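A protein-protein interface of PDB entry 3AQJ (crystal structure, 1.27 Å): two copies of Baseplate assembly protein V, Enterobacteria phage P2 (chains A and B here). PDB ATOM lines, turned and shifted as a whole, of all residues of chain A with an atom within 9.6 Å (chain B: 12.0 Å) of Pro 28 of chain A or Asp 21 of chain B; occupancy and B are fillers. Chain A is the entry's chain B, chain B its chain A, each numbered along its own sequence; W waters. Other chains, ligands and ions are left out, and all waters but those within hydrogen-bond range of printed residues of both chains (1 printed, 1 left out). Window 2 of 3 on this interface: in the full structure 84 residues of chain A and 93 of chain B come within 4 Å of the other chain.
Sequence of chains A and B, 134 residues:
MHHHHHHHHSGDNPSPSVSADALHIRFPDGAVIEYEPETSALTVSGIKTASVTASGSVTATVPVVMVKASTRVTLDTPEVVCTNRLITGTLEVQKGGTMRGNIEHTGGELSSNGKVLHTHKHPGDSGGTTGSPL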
ATOM      1  N   ILE A  25       3.025  17.923   4.762  1.00  0.00           N
ATOM      2  CA  ILE A  25       3.778  19.143   4.849  1.00  0.00           C
ATOM      3  C   ILE A  25       5.279  18.809   4.791  1.00  0.00           C
ATOM      4  O   ILE A  25       5.774  17.907   5.530  1.00  0.00           O
ATOM      5  CB  ILE A  25       3.502  19.861   6.189  1.00  0.00           C
ATOM      6  CG1 ILE A  25       1.998  19.894   6.502  1.00  0.00           C
ATOM      7  CG2 ILE A  25       4.155  21.258   6.262  1.00  0.00           C
ATOM      8  CD1 ILE A  25       1.733  20.635   7.912  1.00  0.00           C
ATOM      9  N   ARG A  26       6.000  19.456   3.903  1.00  0.00           N
ATOM     10  CA  ARG A  26       7.402  19.164   3.666  1.00  0.00           C
ATOM     11  C   ARG A  26       8.250  20.327   3.998  1.00  0.00           C
ATOM     12  O   ARG A  26       7.923  21.466   3.612  1.00  0.00           O
ATOM     13  CB  ARG A  26       7.574  18.839   2.187  1.00  0.00           C
ATOM     14  CG  ARG A  26       6.635  17.774   1.686  1.00  0.00           C
ATOM     15  CD  ARG A  26       6.807  17.618   0.184  1.00  0.00           C
ATOM     16  NE  ARG A  26       5.874  16.614  -0.275  1.00  0.00           N
ATOM     17  CZ  ARG A  26       6.052  15.291  -0.177  1.00  0.00           C
ATOM     18  NH1 ARG A  26       7.134  14.776   0.441  1.00  0.00           N
ATOM     19  NH2 ARG A  26       5.108  14.473  -0.676  1.00  0.00           N
ATOM     20  N   PHE A  27       9.373  20.117   4.599  1.00  0.00           N
ATOM     21  CA  PHE A  27      10.236  21.183   5.042  1.00  0.00           C
ATOM     22  C   PHE A  27      11.580  21.127   4.307  1.00  0.00           C
ATOM     23  O   PHE A  27      12.027  20.121   3.819  1.00  0.00           O
ATOM     24  CB  PHE A  27      10.430  21.026   6.588  1.00  0.00           C
ATOM     25  CG  PHE A  27       9.161  21.152   7.328  1.00  0.00           C
ATOM     26  CD1 PHE A  27       8.589  22.396   7.548  1.00  0.00           C
ATOM     27  CD2 PHE A  27       8.473  20.010   7.744  1.00  0.00           C
ATOM     28  CE1 PHE A  27       7.363  22.487   8.246  1.00  0.00           C
ATOM     29  CE2 PHE A  27       7.250  20.061   8.430  1.00  0.00           C
ATOM     30  CZ  PHE A  27       6.690  21.325   8.680  1.00  0.00           C
ATOM     31  N   PRO A  28      12.330  22.240   4.368  1.00  0.00           N
ATOM     32  CA  PRO A  28      13.575  22.354   3.586  1.00  0.00           C
ATOM     33  C   PRO A  28      14.718  21.479   4.039  1.00  0.00           C
ATOM     34  O   PRO A  28      15.697  21.235   3.292  1.00  0.00           O
ATOM     35  CB  PRO A  28      13.997  23.842   3.778  1.00  0.00           C
ATOM     36  CG  PRO A  28      12.726  24.554   4.351  1.00  0.00           C
ATOM     37  CD  PRO A  28      11.853  23.534   4.999  1.00  0.00           C
ATOM     38  N   ASP A  29      14.638  20.945   5.275  1.00  0.00           N
ATOM     39  CA  ASP A  29      15.639  19.999   5.774  1.00  0.00           C
ATOM     40  C   ASP A  29      15.317  18.515   5.432  1.00  0.00           C
ATOM     41  O   ASP A  29      16.075  17.617   5.869  1.00  0.00           O
ATOM     42  CB  ASP A  29      15.838  20.163   7.302  1.00  0.00           C
ATOM     43  CG  ASP A  29      14.532  19.831   8.094  1.00  0.00           C
ATOM     44  OD1 ASP A  29      13.449  19.701   7.506  1.00  0.00           O
ATOM     45  OD2 ASP A  29      14.682  19.728   9.355  1.00  0.00           O
ATOM     46  N   GLY A  30      14.239  18.284   4.653  1.00  0.00           N
ATOM     47  CA  GLY A  30      13.810  16.950   4.316  1.00  0.00           C
ATOM     48  C   GLY A  30      12.788  16.355   5.276  1.00  0.00           C
ATOM     49  O   GLY A  30      12.314  15.248   5.009  1.00  0.00           O
ATOM     50  N   ALA A  31      12.440  17.066   6.365  1.00  0.00           N
ATOM     51  CA  ALA A  31      11.376  16.540   7.224  1.00  0.00           C
ATOM     52  C   ALA A  31      10.048  16.521   6.517  1.00  0.00           C
ATOM     53  O   ALA A  31       9.761  17.373   5.701  1.00  0.00           O
ATOM     54  CB  ALA A  31      11.343  17.355   8.542  1.00  0.00           C
ATOM     55  N   VAL A  32       9.218  15.597   6.879  1.00  0.00           N
ATOM     56  CA  VAL A  32       7.834  15.453   6.428  1.00  0.00           C
ATOM     57  C   VAL A  32       6.908  15.158   7.592  1.00  0.00           C
ATOM     58  O   VAL A  32       7.223  14.295   8.427  1.00  0.00           O
ATOM     59  CB  VAL A  32       7.666  14.368   5.373  1.00  0.00           C
ATOM     60  CG1 VAL A  32       6.192  14.172   4.838  1.00  0.00           C
ATOM     61  CG2 VAL A  32       8.600  14.717   4.151  1.00  0.00           C
ATOM     62  N   GLY A  46      12.326  12.273   8.952  1.00  0.00           N
ATOM     63  CA  GLY A  46      13.322  13.257   8.532  1.00  0.00           C
ATOM     64  C   GLY A  46      13.636  14.372   9.486  1.00  0.00           C
ATOM     65  O   GLY A  46      14.274  15.353   9.100  1.00  0.00           O
ATOM     66  N   VAL B  18       1.573  22.283   0.804  1.00  0.00           N
ATOM     67  CA  VAL B  18       2.561  21.215   0.441  1.00  0.00           C
ATOM     68  C   VAL B  18       3.942  21.412   0.947  1.00  0.00           C
ATOM     69  O   VAL B  18       4.381  20.723   1.884  1.00  0.00           O
ATOM     70  CB  VAL B  18       2.529  20.603  -0.954  1.00  0.00           C
ATOM     71  CG1 VAL B  18       1.529  19.520  -0.931  1.00  0.00           C
ATOM     72  CG2 VAL B  18       2.433  21.539  -2.017  1.00  0.00           C
ATOM     73  N   SER B  19       4.620  22.363   0.464  1.00  0.00           N
ATOM     74  CA  SER B  19       5.948  22.805   1.012  1.00  0.00           C
ATOM     75  C   SER B  19       5.825  24.005   1.823  1.00  0.00           C
ATOM     76  O   SER B  19       5.174  25.061   1.513  1.00  0.00           O
ATOM     77  CB  SER B  19       7.076  22.859  -0.028  1.00  0.00           C
ATOM     78  OG  SER B  19       8.269  23.479   0.245  1.00  0.00           O
ATOM     79  N   ALA B  20       6.396  23.921   2.916  1.00  0.00           N
ATOM     80  CA  ALA B  20       6.318  25.052   3.947  1.00  0.00           C
ATOM     81  C   ALA B  20       7.724  25.334   4.433  1.00  0.00           C
ATOM     82  O   ALA B  20       8.556  24.403   4.544  1.00  0.00           O
ATOM     83  CB  ALA B  20       5.380  24.670   5.091  1.00  0.00           C
ATOM     84  N   ASP B  21       8.053  26.604   4.713  1.00  0.00           N
ATOM     85  CA  ASP B  21       9.375  27.000   5.207  1.00  0.00           C
ATOM     86  C   ASP B  21       9.642  26.500   6.610  1.00  0.00           C
ATOM     87  O   ASP B  21      10.763  26.127   6.958  1.00  0.00           O
ATOM     88  CB  ASP B  21       9.639  28.519   5.016  1.00  0.00           C
ATOM     89  CG  ASP B  21      10.606  29.120   6.006  1.00  0.00           C
ATOM     90  OD1 ASP B  21      10.751  28.642   7.148  1.00  0.00           O
ATOM     91  OD2 ASP B  21      11.251  30.156   5.643  1.00  0.00           O
ATOM     92  N   ALA B  22       8.596  26.389   7.333  1.00  0.00           N
ATOM     93  CA  ALA B  22       8.646  25.986   8.790  1.00  0.00           C
ATOM     94  C   ALA B  22       7.213  25.818   9.158  1.00  0.00           C
ATOM     95  O   ALA B  22       6.234  25.911   8.360  1.00  0.00           O
ATOM     96  CB  ALA B  22       9.292  27.035   9.658  1.00  0.00           C
ATOM     97  N   LEU B  23       7.042  25.569  10.409  1.00  0.00           N
ATOM     98  CA  LEU B  23       5.651  25.481  10.887  1.00  0.00           C
ATOM     99  C   LEU B  23       5.628  26.158  12.272  1.00  0.00           C
ATOM    100  O   LEU B  23       6.399  25.803  13.140  1.00  0.00           O
ATOM    101  CB  LEU B  23       5.215  24.015  10.941  1.00  0.00           C
ATOM    102  CG  LEU B  23       3.802  23.785  11.512  1.00  0.00           C
ATOM    103  CD1 LEU B  23       2.789  24.426  10.531  1.00  0.00           C
ATOM    104  CD2 LEU B  23       3.587  22.227  11.774  1.00  0.00           C
ATOM    105  N   HIS B  24       4.717  27.098  12.472  1.00  0.00           N
ATOM    106  CA  HIS B  24       4.517  27.639  13.805  1.00  0.00           C
ATOM    107  C   HIS B  24       3.032  27.791  13.920  1.00  0.00           C
ATOM    108  O   HIS B  24       2.384  28.585  13.112  1.00  0.00           O
ATOM    109  CB  HIS B  24       5.206  28.985  13.926  1.00  0.00           C
ATOM    110  CG  HIS B  24       6.681  28.864  13.969  1.00  0.00           C
ATOM    111  ND1 HIS B  24       7.477  28.998  12.845  1.00  0.00           N
ATOM    112  CD2 HIS B  24       7.516  28.581  15.000  1.00  0.00           C
ATOM    113  CE1 HIS B  24       8.753  28.829  13.192  1.00  0.00           C
ATOM    114  NE2 HIS B  24       8.806  28.579  14.493  1.00  0.00           N
ATOM    115  N   ILE B  25       2.396  27.054  14.802  1.00  0.00           N
ATOM    116  CA  ILE B  25       0.972  27.245  15.074  1.00  0.00           C
ATOM    117  C   ILE B  25       0.877  27.589  16.598  1.00  0.00           C
ATOM    118  O   ILE B  25       1.324  26.793  17.454  1.00  0.00           O
ATOM    119  CB  ILE B  25       0.135  26.010  14.819  1.00  0.00           C
ATOM    120  CG1 ILE B  25       0.448  25.473  13.365  1.00  0.00           C
ATOM    121  CG2 ILE B  25      -1.287  26.333  15.001  1.00  0.00           C
ATOM    122  CD1 ILE B  25      -0.186  24.102  13.193  1.00  0.00           C
ATOM    123  N   ILE B  33       2.602  24.436  18.555  1.00  0.00           N
ATOM    124  CA  ILE B  33       3.016  23.278  17.688  1.00  0.00           C
ATOM    125  C   ILE B  33       3.932  23.842  16.675  1.00  0.00           C
ATOM    126  O   ILE B  33       3.523  24.757  15.893  1.00  0.00           O
ATOM    127  CB  ILE B  33       1.834  22.573  17.080  1.00  0.00           C
ATOM    128  CG1 ILE B  33       0.949  22.024  18.161  1.00  0.00           C
ATOM    129  CG2 ILE B  33       2.339  21.450  16.128  1.00  0.00           C
ATOM    130  CD1 ILE B  33      -0.327  21.373  17.588  1.00  0.00           C
ATOM    131  N   GLU B  34       5.166  23.405  16.633  1.00  0.00           N
ATOM    132  CA  GLU B  34       6.140  24.041  15.682  1.00  0.00           C
ATOM    133  C   GLU B  34       7.085  23.032  15.140  1.00  0.00           C
ATOM    134  O   GLU B  34       7.462  22.010  15.772  1.00  0.00           O
ATOM    135  CB  GLU B  34       6.874  25.186  16.346  1.00  0.00           C
ATOM    136  CG  GLU B  34       7.558  24.843  17.491  1.00  0.00           C
ATOM    137  CD  GLU B  34       7.868  26.032  18.349  1.00  0.00           C
ATOM    138  OE1 GLU B  34       7.727  27.169  17.855  1.00  0.00           O
ATOM    139  OE2 GLU B  34       8.161  25.863  19.585  1.00  0.00           O
ATOM    140  N   TYR B  35       7.549  23.284  13.928  1.00  0.00           N
ATOM    141  CA  TYR B  35       8.692  22.585  13.308  1.00  0.00           C
ATOM    142  C   TYR B  35       9.695  23.615  12.824  1.00  0.00           C
ATOM    143  O   TYR B  35       9.341  24.544  11.962  1.00  0.00           O
ATOM    144  CB  TYR B  35       8.276  21.670  12.256  1.00  0.00           C
ATOM    145  CG  TYR B  35       9.519  20.894  11.869  1.00  0.00           C
ATOM    146  CD1 TYR B  35      10.023  19.866  12.751  1.00  0.00           C
ATOM    147  CD2 TYR B  35      10.224  21.154  10.676  1.00  0.00           C
ATOM    148  CE1 TYR B  35      11.203  19.168  12.490  1.00  0.00           C
ATOM    149  CE2 TYR B  35      11.438  20.420  10.395  1.00  0.00           C
ATOM    150  CZ  TYR B  35      11.846  19.474  11.266  1.00  0.00           C
ATOM    151  OH  TYR B  35      13.034  18.738  11.064  1.00  0.00           O
ATOM    152  N   GLU B  36      10.939  23.564  13.320  1.00  0.00           N
ATOM    153  CA  GLU B  36      11.988  24.493  12.990  1.00  0.00           C
ATOM    154  C   GLU B  36      13.041  23.782  12.213  1.00  0.00           C
ATOM    155  O   GLU B  36      13.835  23.046  12.783  1.00  0.00           O
ATOM    156  CB  GLU B  36      12.624  25.121  14.265  1.00  0.00           C
ATOM    157  CG  GLU B  36      13.741  26.199  13.917  1.00  0.00           C
ATOM    158  CD  GLU B  36      13.318  27.132  12.799  1.00  0.00           C
ATOM    159  OE1 GLU B  36      12.337  27.885  13.014  1.00  0.00           O
ATOM    160  OE2 GLU B  36      13.911  27.161  11.697  1.00  0.00           O
ATOM    161  N   PRO B  37      13.126  24.022  10.905  1.00  0.00           N
ATOM    162  CA  PRO B  37      14.165  23.297  10.081  1.00  0.00           C
ATOM    163  C   PRO B  37      15.589  23.684  10.434  1.00  0.00           C
ATOM    164  O   PRO B  37      16.460  22.842  10.209  1.00  0.00           O
ATOM    165  CB  PRO B  37      13.838  23.690   8.640  1.00  0.00           C
ATOM    166  CG  PRO B  37      12.336  23.985   8.666  1.00  0.00           C
ATOM    167  CD  PRO B  37      12.090  24.699  10.087  1.00  0.00           C
ATOM    168  N   GLU B  38      15.865  24.833  11.056  1.00  0.00           N
ATOM    169  CA  GLU B  38      17.227  25.207  11.356  1.00  0.00           C
ATOM    170  C   GLU B  38      17.835  24.234  12.363  1.00  0.00           C
ATOM    171  O   GLU B  38      18.979  23.766  12.228  1.00  0.00           O
ATOM    172  CB  GLU B  38      17.240  26.633  11.937  1.00  0.00           C
ATOM    173  CG  GLU B  38      18.592  27.188  12.257  1.00  0.00           C
ATOM    174  CD  GLU B  38      18.476  28.498  13.023  1.00  0.00           C
ATOM    175  OE1 GLU B  38      19.267  28.633  14.001  1.00  0.00           O
ATOM    176  OE2 GLU B  38      17.578  29.357  12.680  1.00  0.00           O
ATOM    177  N   THR B  39      17.057  23.861  13.376  1.00  0.00           N
ATOM    178  CA  THR B  39      17.504  22.943  14.416  1.00  0.00           C
ATOM    179  C   THR B  39      16.912  21.567  14.123  1.00  0.00           C
ATOM    180  O   THR B  39      17.275  20.605  14.835  1.00  0.00           O
ATOM    181  CB  THR B  39      17.011  23.417  15.768  1.00  0.00           C
ATOM    182  OG1 THR B  39      15.579  23.524  15.625  1.00  0.00           O
ATOM    183  CG2 THR B  39      17.713  24.749  16.153  1.00  0.00           C
ATOM    184  N   SER B  40      16.019  21.421  13.153  1.00  0.00           N
ATOM    185  CA  SER B  40      15.314  20.190  12.786  1.00  0.00           C
ATOM    186  C   SER B  40      14.491  19.639  14.015  1.00  0.00           C
ATOM    187  O   SER B  40      14.459  18.425  14.247  1.00  0.00           O
ATOM    188  CB  SER B  40      16.242  19.167  12.190  1.00  0.00           C
ATOM    189  OG  SER B  40      16.849  19.729  10.999  1.00  0.00           O
ATOM    190  N   ALA B  41      13.869  20.561  14.720  1.00  0.00           N
ATOM    191  CA  ALA B  41      13.155  20.216  15.970  1.00  0.00           C
ATOM    192  C   ALA B  41      11.613  20.352  15.797  1.00  0.00           C
ATOM    193  O   ALA B  41      11.131  21.416  15.389  1.00  0.00           O
ATOM    194  CB  ALA B  41      13.566  21.105  17.020  1.00  0.00           C
ATOM    195  N   LEU B  42      10.878  19.277  16.074  1.00  0.00           N
ATOM    196  CA  LEU B  42       9.396  19.341  16.219  1.00  0.00           C
ATOM    197  C   LEU B  42       9.074  19.478  17.644  1.00  0.00           C
ATOM    198  O   LEU B  42       9.598  18.714  18.499  1.00  0.00           O
ATOM    199  CB  LEU B  42       8.826  18.049  15.695  1.00  0.00           C
ATOM    200  CG  LEU B  42       7.334  17.822  15.888  1.00  0.00           C
ATOM    201  CD1 LEU B  42       6.561  18.850  15.132  1.00  0.00           C
ATOM    202  CD2 LEU B  42       6.884  16.375  15.499  1.00  0.00           C
HETATM  203  O   HOH W   1      16.564  16.536  10.093  1.00  0.00           O
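Position printed for both chains: 25. Of the 16 pairs that touch across the chains among the printed residues, none has its exchanged pair printed and touching as well.
N of Tyr 35 of chain B sits at hydrogen-bond distance from O of Leu 23 of chain B, at 2.9 Å. OG of Ser 40 of chain B lies within hydrogen-bond range of O of Pro 37 of chain B (3.2 Å). OD1 of Asp 29 of chain A lies within hydrogen-bond range of N of Ala 31 of chain A.
The backbone carbonyl oxygen (O) of Val 18 of chain B lies within hydrogen-bond range of the backbone NH (N) of Arg 26 of chain A, 2.9 Å away. The backbone carbonyl oxygen of Arg 26 of chain A is in hydrogen-bond range of the backbone NH of Ala 20 of chain B (3.0 Å). The side-chain hydroxyl of Tyr 35 of chain B lies within hydrogen-bond range of the side-chain carboxylate of Asp 29 of chain A (2.6 Å). OG of Ser 40 of chain B sits at hydrogen-bond distance from OD2 of Asp 29 of chain A.
Water W1 lies within hydrogen-bond range of the backbone carbonyl oxygen (O) of Gly 46 of chain A (2.8 Å) and the side-chain hydroxyl (OG) of Ser 40 of chain B (3.3 Å).
Val 18 of chain B touches Ile 25 of chain A. CG2 of Ile 25 of chain A touches CB of Ala 20 of chain B, at 3.8 Å. O of Arg 26 of chain A touches CA of Ser 19 of chain B, at 3.5 Å. Phe 27 of chain A touches Ala 20 of chain B (CD1 to O, 3.6 Å). CE1 of Phe 27 of chain A touches C of Ala 22 of chain B, 3.5 Å away. CE1 of Phe 27 of chain A touches CB of Leu 23 of chain B, 3.8 Å away. Tyr 35 of chain B touches Phe 27 of chain A (CD2 to CG, 3.5 Å). Ala 20 of chain B touches Pro 28 of chain A. Pro 28 of chain A touches Asp 21 of chain B (CD to O, 3.4 Å). Ala 31 of chain A touches Tyr 35 of chain B (CB to OH, 3.3 Å).
Of the printed residues of chain B, Pro 28 of chain A touches Ala 20, Asp 21 and Pro 37. Printed residues of chain A within 4 Å of Asp 21 of chain B: Pro 28 (3.4 Å). Of chain B, only Ala 20 (3.6 Å), Ala 22 (3.5 Å), Leu 23 (3.8 Å) and Tyr 35 (3.5 Å) come within 4 Å of Phe 27 of chain A. Asp 29 of chain A touches just these residues of chain B: Tyr 35, Pro 37 and Ser 40. No residue of chain B comes within 4 Å of Gly 30 of chain A. Ala 22 of chain B touches just one residue of chain A: Phe 27. Of the printed residues of chain A, Val 18 of chain B touches Ile 25 (3.4 Å) and Arg 26 (2.9 Å). Of the printed residues of chain A, Ser 40 of chain B touches Asp 29 (2.7 Å). Printed residues of chain A within 4 Å of Tyr 35 of chain B: Phe 27 (3.5 Å), Asp 29 (2.6 Å) and Ala 31 (3.3 Å). Of the printed residues of chain B, Arg 26 of chain A touches Val 18, Ser 19 and Ala 20. Of the printed residues of chain A, Pro 37 of chain B touches Pro 28 and Asp 29. Ile 25 of chain B touches none of the printed residues of chain A. The nearest printed residue of chain A that does not touch Val 18 of chain B is Phe 27 of chain A (5.7 Å).
Hydrophobic or aromatic side chains of chain B that line the printed part of chain A: Ala 20, Leu 23, Tyr 35 and Pro 37. Along chain B the printed residues that touch a printed residue of chain A span positions 18 to 40. Of the 9 printed residues of chain A, 6 touch a printed residue of chain B. Among the printed residues, 16 pairs touch across the chains.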
